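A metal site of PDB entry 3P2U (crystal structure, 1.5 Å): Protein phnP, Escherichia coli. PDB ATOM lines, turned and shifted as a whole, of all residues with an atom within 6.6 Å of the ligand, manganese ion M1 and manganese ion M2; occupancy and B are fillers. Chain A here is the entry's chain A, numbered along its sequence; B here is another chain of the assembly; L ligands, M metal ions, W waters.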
ATOM      1  N   GLY A  11      -5.304 -37.567 -16.958  1.00  0.00           N
ATOM      2  CA  GLY A  11      -4.079 -36.785 -17.017  1.00  0.00           C
ATOM      3  C   GLY A  11      -4.323 -35.291 -16.992  1.00  0.00           C
ATOM      4  O   GLY A  11      -5.451 -34.822 -16.951  1.00  0.00           O
ATOM      5  N   GLY A  12      -3.233 -34.534 -17.012  1.00  0.00           N
ATOM      6  CA  GLY A  12      -3.331 -33.099 -17.221  1.00  0.00           C
ATOM      7  C   GLY A  12      -3.058 -32.752 -18.663  1.00  0.00           C
ATOM      8  O   GLY A  12      -3.048 -33.621 -19.541  1.00  0.00           O
ATOM      9  N   ALA A  13      -2.850 -31.476 -18.920  1.00  0.00           N
ATOM     10  CA  ALA A  13      -2.654 -30.991 -20.275  1.00  0.00           C
ATOM     11  C   ALA A  13      -1.496 -31.681 -21.010  1.00  0.00           C
ATOM     12  O   ALA A  13      -1.569 -31.990 -22.205  1.00  0.00           O
ATOM     13  CB  ALA A  13      -2.436 -29.484 -20.255  1.00  0.00           C
ATOM     14  N   GLN A  14      -0.418 -31.933 -20.275  1.00  0.00           N
ATOM     15  CA  GLN A  14       0.782 -32.555 -20.820  1.00  0.00           C
ATOM     16  C   GLN A  14       0.563 -34.019 -21.188  1.00  0.00           C
ATOM     17  O   GLN A  14       1.167 -34.537 -22.126  1.00  0.00           O
ATOM     18  CB  GLN A  14       1.895 -32.414 -19.798  1.00  0.00           C
ATOM     19  CG  GLN A  14       3.226 -33.085 -20.138  1.00  0.00           C
ATOM     20  CD  GLN A  14       4.230 -32.871 -19.025  1.00  0.00           C
ATOM     21  OE1 GLN A  14       3.982 -33.264 -17.875  1.00  0.00           O
ATOM     22  NE2 GLN A  14       5.344 -32.220 -19.327  1.00  0.00           N
ATOM     23  N   CYS A  40      -8.134 -34.751 -18.349  1.00  0.00           N
ATOM     24  CA  CYS A  40      -9.068 -34.978 -17.260  1.00  0.00           C
ATOM     25  C   CYS A  40     -10.521 -34.711 -17.647  1.00  0.00           C
ATOM     26  O   CYS A  40     -10.911 -33.572 -17.884  1.00  0.00           O
ATOM     27  CB  CYS A  40      -8.680 -34.085 -16.087  1.00  0.00           C
ATOM     28  SG  CYS A  40      -9.639 -34.369 -14.598  1.00  0.00           S
ATOM     29  N   HIS A  76     -14.119 -25.538 -16.281  1.00  0.00           N
ATOM     30  CA  HIS A  76     -13.478 -24.282 -16.628  1.00  0.00           C
ATOM     31  C   HIS A  76     -13.025 -24.322 -18.071  1.00  0.00           C
ATOM     32  O   HIS A  76     -13.124 -25.366 -18.712  1.00  0.00           O
ATOM     33  CB  HIS A  76     -12.308 -23.933 -15.680  1.00  0.00           C
ATOM     34  CG  HIS A  76     -11.118 -24.845 -15.771  1.00  0.00           C
ATOM     35  ND1 HIS A  76     -11.194 -26.214 -15.559  1.00  0.00           N
ATOM     36  CD2 HIS A  76      -9.796 -24.572 -15.922  1.00  0.00           C
ATOM     37  CE1 HIS A  76      -9.979 -26.738 -15.605  1.00  0.00           C
ATOM     38  NE2 HIS A  76      -9.116 -25.757 -15.818  1.00  0.00           N
ATOM     39  N   HIS A  78      -9.964 -23.644 -19.545  1.00  0.00           N
ATOM     40  CA  HIS A  78      -8.624 -23.982 -20.021  1.00  0.00           C
ATOM     41  C   HIS A  78      -8.733 -24.926 -21.214  1.00  0.00           C
ATOM     42  O   HIS A  78      -9.644 -25.758 -21.310  1.00  0.00           O
ATOM     43  CB  HIS A  78      -7.773 -24.625 -18.928  1.00  0.00           C
ATOM     44  CG  HIS A  78      -7.041 -23.632 -18.073  1.00  0.00           C
ATOM     45  ND1 HIS A  78      -6.799 -23.836 -16.734  1.00  0.00           N
ATOM     46  CD2 HIS A  78      -6.511 -22.423 -18.377  1.00  0.00           C
ATOM     47  CE1 HIS A  78      -6.137 -22.800 -16.243  1.00  0.00           C
ATOM     48  NE2 HIS A  78      -5.957 -21.932 -17.226  1.00  0.00           N
ATOM     49  N   MET A  79      -7.786 -24.804 -22.137  1.00  0.00           N
ATOM     50  CA  MET A  79      -7.860 -25.543 -23.385  1.00  0.00           C
ATOM     51  C   MET A  79      -7.978 -27.043 -23.219  1.00  0.00           C
ATOM     52  O   MET A  79      -8.710 -27.685 -23.972  1.00  0.00           O
ATOM     53  CB  MET A  79      -6.650 -25.214 -24.269  1.00  0.00           C
ATOM     54  CG  MET A  79      -6.736 -25.789 -25.685  1.00  0.00           C
ATOM     55  SD  MET A  79      -8.162 -25.177 -26.643  1.00  0.00           S
ATOM     56  CE  MET A  79      -7.534 -23.568 -27.119  1.00  0.00           C
ATOM     57  N   ASP A  80      -7.266 -27.603 -22.235  1.00  0.00           N
ATOM     58  CA  ASP A  80      -7.272 -29.057 -22.041  1.00  0.00           C
ATOM     59  C   ASP A  80      -8.597 -29.572 -21.488  1.00  0.00           C
ATOM     60  O   ASP A  80      -8.765 -30.775 -21.316  1.00  0.00           O
ATOM     61  CB  ASP A  80      -6.083 -29.549 -21.188  1.00  0.00           C
ATOM     62  CG  ASP A  80      -6.033 -28.931 -19.794  1.00  0.00           C
ATOM     63  OD1 ASP A  80      -6.163 -27.705 -19.675  1.00  0.00           O
ATOM     64  OD2 ASP A  80      -5.876 -29.684 -18.801  1.00  0.00           O
ATOM     65  N   HIS A  81      -9.535 -28.661 -21.206  1.00  0.00           N
ATOM     66  CA  HIS A  81     -10.880 -29.057 -20.787  1.00  0.00           C
ATOM     67  C   HIS A  81     -11.966 -28.732 -21.805  1.00  0.00           C
ATOM     68  O   HIS A  81     -13.123 -29.160 -21.639  1.00  0.00           O
ATOM     69  CB  HIS A  81     -11.209 -28.435 -19.421  1.00  0.00           C
ATOM     70  CG  HIS A  81     -10.283 -28.885 -18.337  1.00  0.00           C
ATOM     71  ND1 HIS A  81     -10.624 -29.814 -17.380  1.00  0.00           N
ATOM     72  CD2 HIS A  81      -8.965 -28.603 -18.122  1.00  0.00           C
ATOM     73  CE1 HIS A  81      -9.592 -30.044 -16.587  1.00  0.00           C
ATOM     74  NE2 HIS A  81      -8.561 -29.328 -17.045  1.00  0.00           N
ATOM     75  N   HIS A 143      -8.019 -21.904  -8.593  1.00  0.00           N
ATOM     76  CA  HIS A 143      -7.394 -22.131  -9.895  1.00  0.00           C
ATOM     77  C   HIS A 143      -7.239 -20.802 -10.637  1.00  0.00           C
ATOM     78  O   HIS A 143      -7.907 -19.821 -10.306  1.00  0.00           O
ATOM     79  CB  HIS A 143      -8.269 -23.093 -10.723  1.00  0.00           C
ATOM     80  CG  HIS A 143      -7.544 -23.829 -11.804  1.00  0.00           C
ATOM     81  ND1 HIS A 143      -6.388 -24.555 -11.570  1.00  0.00           N
ATOM     82  CD2 HIS A 143      -7.826 -23.986 -13.121  1.00  0.00           C
ATOM     83  CE1 HIS A 143      -5.990 -25.114 -12.699  1.00  0.00           C
ATOM     84  NE2 HIS A 143      -6.837 -24.785 -13.655  1.00  0.00           N
ATOM     85  N   SER A 144      -6.380 -20.770 -11.647  1.00  0.00           N
ATOM     86  CA  SER A 144      -6.061 -19.512 -12.331  1.00  0.00           C
ATOM     87  C   SER A 144      -7.207 -18.993 -13.204  1.00  0.00           C
ATOM     88  O   SER A 144      -7.225 -17.826 -13.600  1.00  0.00           O
ATOM     89  CB  SER A 144      -4.778 -19.665 -13.150  1.00  0.00           C
ATOM     90  OG  SER A 144      -4.896 -20.736 -14.067  1.00  0.00           O
ATOM     91  N   LYS A 145      -8.147 -19.877 -13.539  1.00  0.00           N
ATOM     92  CA  LYS A 145      -9.379 -19.513 -14.214  1.00  0.00           C
ATOM     93  C   LYS A 145     -10.552 -19.683 -13.269  1.00  0.00           C
ATOM     94  O   LYS A 145     -10.451 -20.438 -12.303  1.00  0.00           O
ATOM     95  CB  LYS A 145      -9.635 -20.461 -15.386  1.00  0.00           C
ATOM     96  CG  LYS A 145      -8.649 -20.347 -16.516  1.00  0.00           C
ATOM     97  CD  LYS A 145      -9.159 -19.369 -17.528  1.00  0.00           C
ATOM     98  CE  LYS A 145      -8.461 -19.563 -18.851  1.00  0.00           C
ATOM     99  NZ  LYS A 145      -8.875 -18.509 -19.799  1.00  0.00           N
ATOM    100  N   THR A 147     -13.236 -21.517 -11.934  1.00  0.00           N
ATOM    101  CA  THR A 147     -13.324 -22.970 -12.038  1.00  0.00           C
ATOM    102  C   THR A 147     -14.286 -23.518 -10.993  1.00  0.00           C
ATOM    103  O   THR A 147     -14.186 -23.156  -9.813  1.00  0.00           O
ATOM    104  CB  THR A 147     -11.928 -23.591 -11.788  1.00  0.00           C
ATOM    105  OG1 THR A 147     -10.994 -23.032 -12.728  1.00  0.00           O
ATOM    106  CG2 THR A 147     -11.961 -25.121 -11.938  1.00  0.00           C
ATOM    107  N   SER A 163     -11.627 -31.106  -9.981  1.00  0.00           N
ATOM    108  CA  SER A 163     -10.423 -30.724 -10.735  1.00  0.00           C
ATOM    109  C   SER A 163     -10.876 -29.538 -11.579  1.00  0.00           C
ATOM    110  O   SER A 163     -12.041 -29.521 -12.006  1.00  0.00           O
ATOM    111  CB  SER A 163      -9.995 -31.895 -11.611  1.00  0.00           C
ATOM    112  OG  SER A 163      -8.596 -31.842 -11.903  1.00  0.00           O
ATOM    113  N   ASP A 164     -10.019 -28.548 -11.850  1.00  0.00           N
ATOM    114  CA  ASP A 164      -8.627 -28.438 -11.373  1.00  0.00           C
ATOM    115  C   ASP A 164      -8.585 -27.538 -10.149  1.00  0.00           C
ATOM    116  O   ASP A 164      -9.268 -26.510 -10.105  1.00  0.00           O
ATOM    117  CB  ASP A 164      -7.794 -27.718 -12.422  1.00  0.00           C
ATOM    118  CG  ASP A 164      -7.660 -28.482 -13.731  1.00  0.00           C
ATOM    119  OD1 ASP A 164      -8.168 -29.610 -13.904  1.00  0.00           O
ATOM    120  OD2 ASP A 164      -6.990 -27.899 -14.594  1.00  0.00           O
ATOM    121  N   ASP A 187      -8.183 -33.624  -8.131  1.00  0.00           N
ATOM    122  CA  ASP A 187      -6.919 -33.204  -8.733  1.00  0.00           C
ATOM    123  C   ASP A 187      -5.773 -33.537  -7.802  1.00  0.00           C
ATOM    124  O   ASP A 187      -5.718 -33.052  -6.671  1.00  0.00           O
ATOM    125  CB  ASP A 187      -6.975 -31.700  -8.945  1.00  0.00           C
ATOM    126  CG  ASP A 187      -5.797 -31.148  -9.753  1.00  0.00           C
ATOM    127  OD1 ASP A 187      -4.743 -31.814  -9.888  1.00  0.00           O
ATOM    128  OD2 ASP A 187      -5.937 -30.030 -10.247  1.00  0.00           O
ATOM    129  N   SER A 189      -2.095 -33.498  -9.118  1.00  0.00           N
ATOM    130  CA  SER A 189      -1.176 -33.469 -10.244  1.00  0.00           C
ATOM    131  C   SER A 189       0.208 -33.923  -9.808  1.00  0.00           C
ATOM    132  O   SER A 189       0.900 -34.600 -10.563  1.00  0.00           O
ATOM    133  CB  SER A 189      -1.102 -32.057 -10.805  1.00  0.00           C
ATOM    134  OG  SER A 189      -2.337 -31.667 -11.385  1.00  0.00           O
ATOM    135  N   ASN A 199      -1.515 -24.094  -8.634  1.00  0.00           N
ATOM    136  CA  ASN A 199      -2.666 -24.269  -9.527  1.00  0.00           C
ATOM    137  C   ASN A 199      -3.295 -25.673  -9.395  1.00  0.00           C
ATOM    138  O   ASN A 199      -4.449 -25.881  -9.766  1.00  0.00           O
ATOM    139  CB  ASN A 199      -2.251 -24.014 -10.984  1.00  0.00           C
ATOM    140  CG  ASN A 199      -3.241 -23.116 -11.754  1.00  0.00           C
ATOM    141  OD1 ASN A 199      -3.297 -23.165 -12.984  1.00  0.00           O
ATOM    142  ND2 ASN A 199      -3.984 -22.286 -11.034  1.00  0.00           N
ATOM    143  N   HIS A 200      -2.500 -26.610  -8.868  1.00  0.00           N
ATOM    144  CA  HIS A 200      -2.958 -27.991  -8.667  1.00  0.00           C
ATOM    145  C   HIS A 200      -2.429 -28.529  -7.360  1.00  0.00           C
ATOM    146  O   HIS A 200      -1.367 -28.111  -6.901  1.00  0.00           O
ATOM    147  CB  HIS A 200      -2.450 -28.895  -9.795  1.00  0.00           C
ATOM    148  CG  HIS A 200      -2.893 -28.472 -11.156  1.00  0.00           C
ATOM    149  ND1 HIS A 200      -4.138 -28.785 -11.666  1.00  0.00           N
ATOM    150  CD2 HIS A 200      -2.258 -27.765 -12.110  1.00  0.00           C
ATOM    151  CE1 HIS A 200      -4.242 -28.273 -12.880  1.00  0.00           C
ATOM    152  NE2 HIS A 200      -3.122 -27.655 -13.177  1.00  0.00           N
ATOM    153  N   HIS A 222      -6.017 -36.134 -12.775  1.00  0.00           N
ATOM    154  CA  HIS A 222      -5.175 -35.055 -13.317  1.00  0.00           C
ATOM    155  C   HIS A 222      -3.687 -35.326 -12.993  1.00  0.00           C
ATOM    156  O   HIS A 222      -2.925 -34.410 -12.670  1.00  0.00           O
ATOM    157  CB  HIS A 222      -5.645 -33.689 -12.794  1.00  0.00           C
ATOM    158  CG  HIS A 222      -5.384 -32.553 -13.735  1.00  0.00           C
ATOM    159  ND1 HIS A 222      -4.160 -31.937 -13.838  1.00  0.00           N
ATOM    160  CD2 HIS A 222      -6.200 -31.889 -14.594  1.00  0.00           C
ATOM    161  CE1 HIS A 222      -4.224 -30.957 -14.724  1.00  0.00           C
ATOM    162  NE2 HIS A 222      -5.448 -30.915 -15.204  1.00  0.00           N
ATOM    163  N   ARG B  89       3.332 -28.661 -26.691  1.00  0.00           N
ATOM    164  CA  ARG B  89       4.188 -27.623 -26.134  1.00  0.00           C
ATOM    165  C   ARG B  89       4.790 -28.002 -24.779  1.00  0.00           C
ATOM    166  O   ARG B  89       5.833 -27.490 -24.386  1.00  0.00           O
ATOM    167  CB  ARG B  89       3.423 -26.303 -26.039  1.00  0.00           C
ATOM    168  CG  ARG B  89       2.203 -26.386 -25.139  1.00  0.00           C
ATOM    169  CD  ARG B  89       1.440 -25.070 -25.136  1.00  0.00           C
ATOM    170  NE  ARG B  89       0.141 -25.239 -24.495  1.00  0.00           N
ATOM    171  CZ  ARG B  89      -0.567 -24.246 -23.986  1.00  0.00           C
ATOM    172  NH1 ARG B  89      -0.100 -23.004 -24.037  1.00  0.00           N
ATOM    173  NH2 ARG B  89      -1.758 -24.488 -23.436  1.00  0.00           N
ATOM    174  N   TRP B  90       4.120 -28.916 -24.066  1.00  0.00           N
ATOM    175  CA  TRP B  90       4.550 -29.315 -22.740  1.00  0.00           C
ATOM    176  C   TRP B  90       5.591 -30.432 -22.798  1.00  0.00           C
ATOM    177  O   TRP B  90       5.945 -31.025 -21.768  1.00  0.00           O
ATOM    178  CB  TRP B  90       3.332 -29.774 -21.925  1.00  0.00           C
ATOM    179  CG  TRP B  90       2.204 -28.790 -21.849  1.00  0.00           C
ATOM    180  CD1 TRP B  90       0.934 -28.955 -22.295  1.00  0.00           C
ATOM    181  CD2 TRP B  90       2.260 -27.462 -21.305  1.00  0.00           C
ATOM    182  NE1 TRP B  90       0.184 -27.826 -22.067  1.00  0.00           N
ATOM    183  CE2 TRP B  90       0.979 -26.904 -21.441  1.00  0.00           C
ATOM    184  CE3 TRP B  90       3.265 -26.694 -20.719  1.00  0.00           C
ATOM    185  CZ2 TRP B  90       0.671 -25.602 -21.023  1.00  0.00           C
ATOM    186  CZ3 TRP B  90       2.967 -25.411 -20.294  1.00  0.00           C
ATOM    187  CH2 TRP B  90       1.677 -24.877 -20.453  1.00  0.00           C
ATOM    188  N   ASP B 109      -3.602 -19.407 -24.973  1.00  0.00           N
ATOM    189  CA  ASP B 109      -2.366 -19.057 -24.265  1.00  0.00           C
ATOM    190  C   ASP B 109      -1.068 -19.628 -24.852  1.00  0.00           C
ATOM    191  O   ASP B 109      -0.080 -19.799 -24.138  1.00  0.00           O
ATOM    192  CB  ASP B 109      -2.466 -19.365 -22.770  1.00  0.00           C
ATOM    193  CG  ASP B 109      -2.494 -20.841 -22.466  1.00  0.00           C
ATOM    194  OD1 ASP B 109      -2.541 -21.647 -23.412  1.00  0.00           O
ATOM    195  OD2 ASP B 109      -2.467 -21.194 -21.273  1.00  0.00           O
HETATM  196  V1  LIG L   1      -3.725 -26.827 -16.261  1.00  0.00           V
HETATM  197  O1  LIG L   1      -4.799 -25.667 -15.201  1.00  0.00           O
HETATM  198  O2  LIG L   1      -4.411 -28.603 -16.352  1.00  0.00           O
HETATM  199  O3  LIG L   1      -3.592 -26.125 -18.026  1.00  0.00           O
HETATM  200  O4  LIG L   1      -1.990 -26.881 -15.451  1.00  0.00           O
HETATM  201 MN    MN M   1      -6.939 -25.663 -15.590  1.00  0.00          MN
HETATM  202 MN    MN M   2      -6.379 -29.053 -16.416  1.00  0.00          MN
HETATM  203  O   HOH W   1      -4.347 -25.974 -21.044  1.00  0.00           O
HETATM  204  O   HOH W   2      -6.403 -26.867 -17.190  1.00  0.00           O
HETATM  205  O   HOH W   3      -2.252 -29.512 -16.929  1.00  0.00           O
HETATM  206  O   HOH W   4      -2.639 -23.716 -17.814  1.00  0.00           O
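O4 of the ligand sits close to NE2 of His 200.
Asn 199 touches the ligand. Hydrophobic or aromatic side chains that line the ligand: His 78, His 143, His 200 and His 222. Of the 24 residues printed, 7 come within 4 Å of the ligand. The nearest printed residue that does not touch the ligand is Ala 13 (4.2 Å).
O of Asn 199 is in hydrogen-bond range of ND1 of His 143 (3.0 Å). A ring nitrogen (ND1) of His 200 sits close to the side-chain hydroxyl of Ser 189 (3.4 Å). The side-chain amide nitrogen of Asn 199 lies close to the backbone NH of Ser 144, at 2.9 Å. The side-chain carboxylate of Asp 187 lies within hydrogen-bond range of a ring nitrogen (ND1) of His 200, 2.6 Å away. A ring nitrogen (ND1) of His 222 lies within hydrogen-bond range of the side-chain hydroxyl (OG) of Ser 189 (3.1 Å). The side-chain hydroxyl of Ser 163 sits at hydrogen-bond distance from the side-chain carboxylate of Asp 164, at 3.0 Å.
Of the 24 residues printed, 4 come within 4 Å of manganese ion M1. Along chain A the residues within 4 Å of manganese ion M1 span positions 76 to 164. The nearest printed residue that does not touch manganese ion M1 is His 81 (4.3 Å).
Manganese ion M2 is bound by an oxygen (O2) of the ligand, at 2.0 Å. The side-chain carboxylate (OD2) of Asp 164 is bound to manganese ion M2 (2.2 Å). Manganese ion M2 is bound by a ring nitrogen (NE2) of His 81, 2.3 Å away. Water W2 binds manganese ion M2, at 2.3 Å. Manganese ion M2 is bound by NE2 of His 222 (2.4 Å). OD2 of Asp 80 is bound to manganese ion M2 (2.5 Å).
Of the 24 residues printed, 4 come within 4 Å of manganese ion M2. The nearest printed residue that does not touch manganese ion M2 is His 200 (4.2 Å).
Water W2 is bound to manganese ion M1 (2.1 Å). Manganese ion M1 is bound by NE2 of His 143 (2.1 Å). Manganese ion M1 is bound by a ring nitrogen (ND1) of His 78, at 2.2 Å. O1 of the ligand is bound to manganese ion M1, at 2.2 Å. NE2 of His 76 binds manganese ion M1, at 2.2 Å. The side-chain carboxylate (OD2) of Asp 164 is bound to manganese ion M1, 2.4 Å away. Manganese ion M1 has six donor atoms within binding distance.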
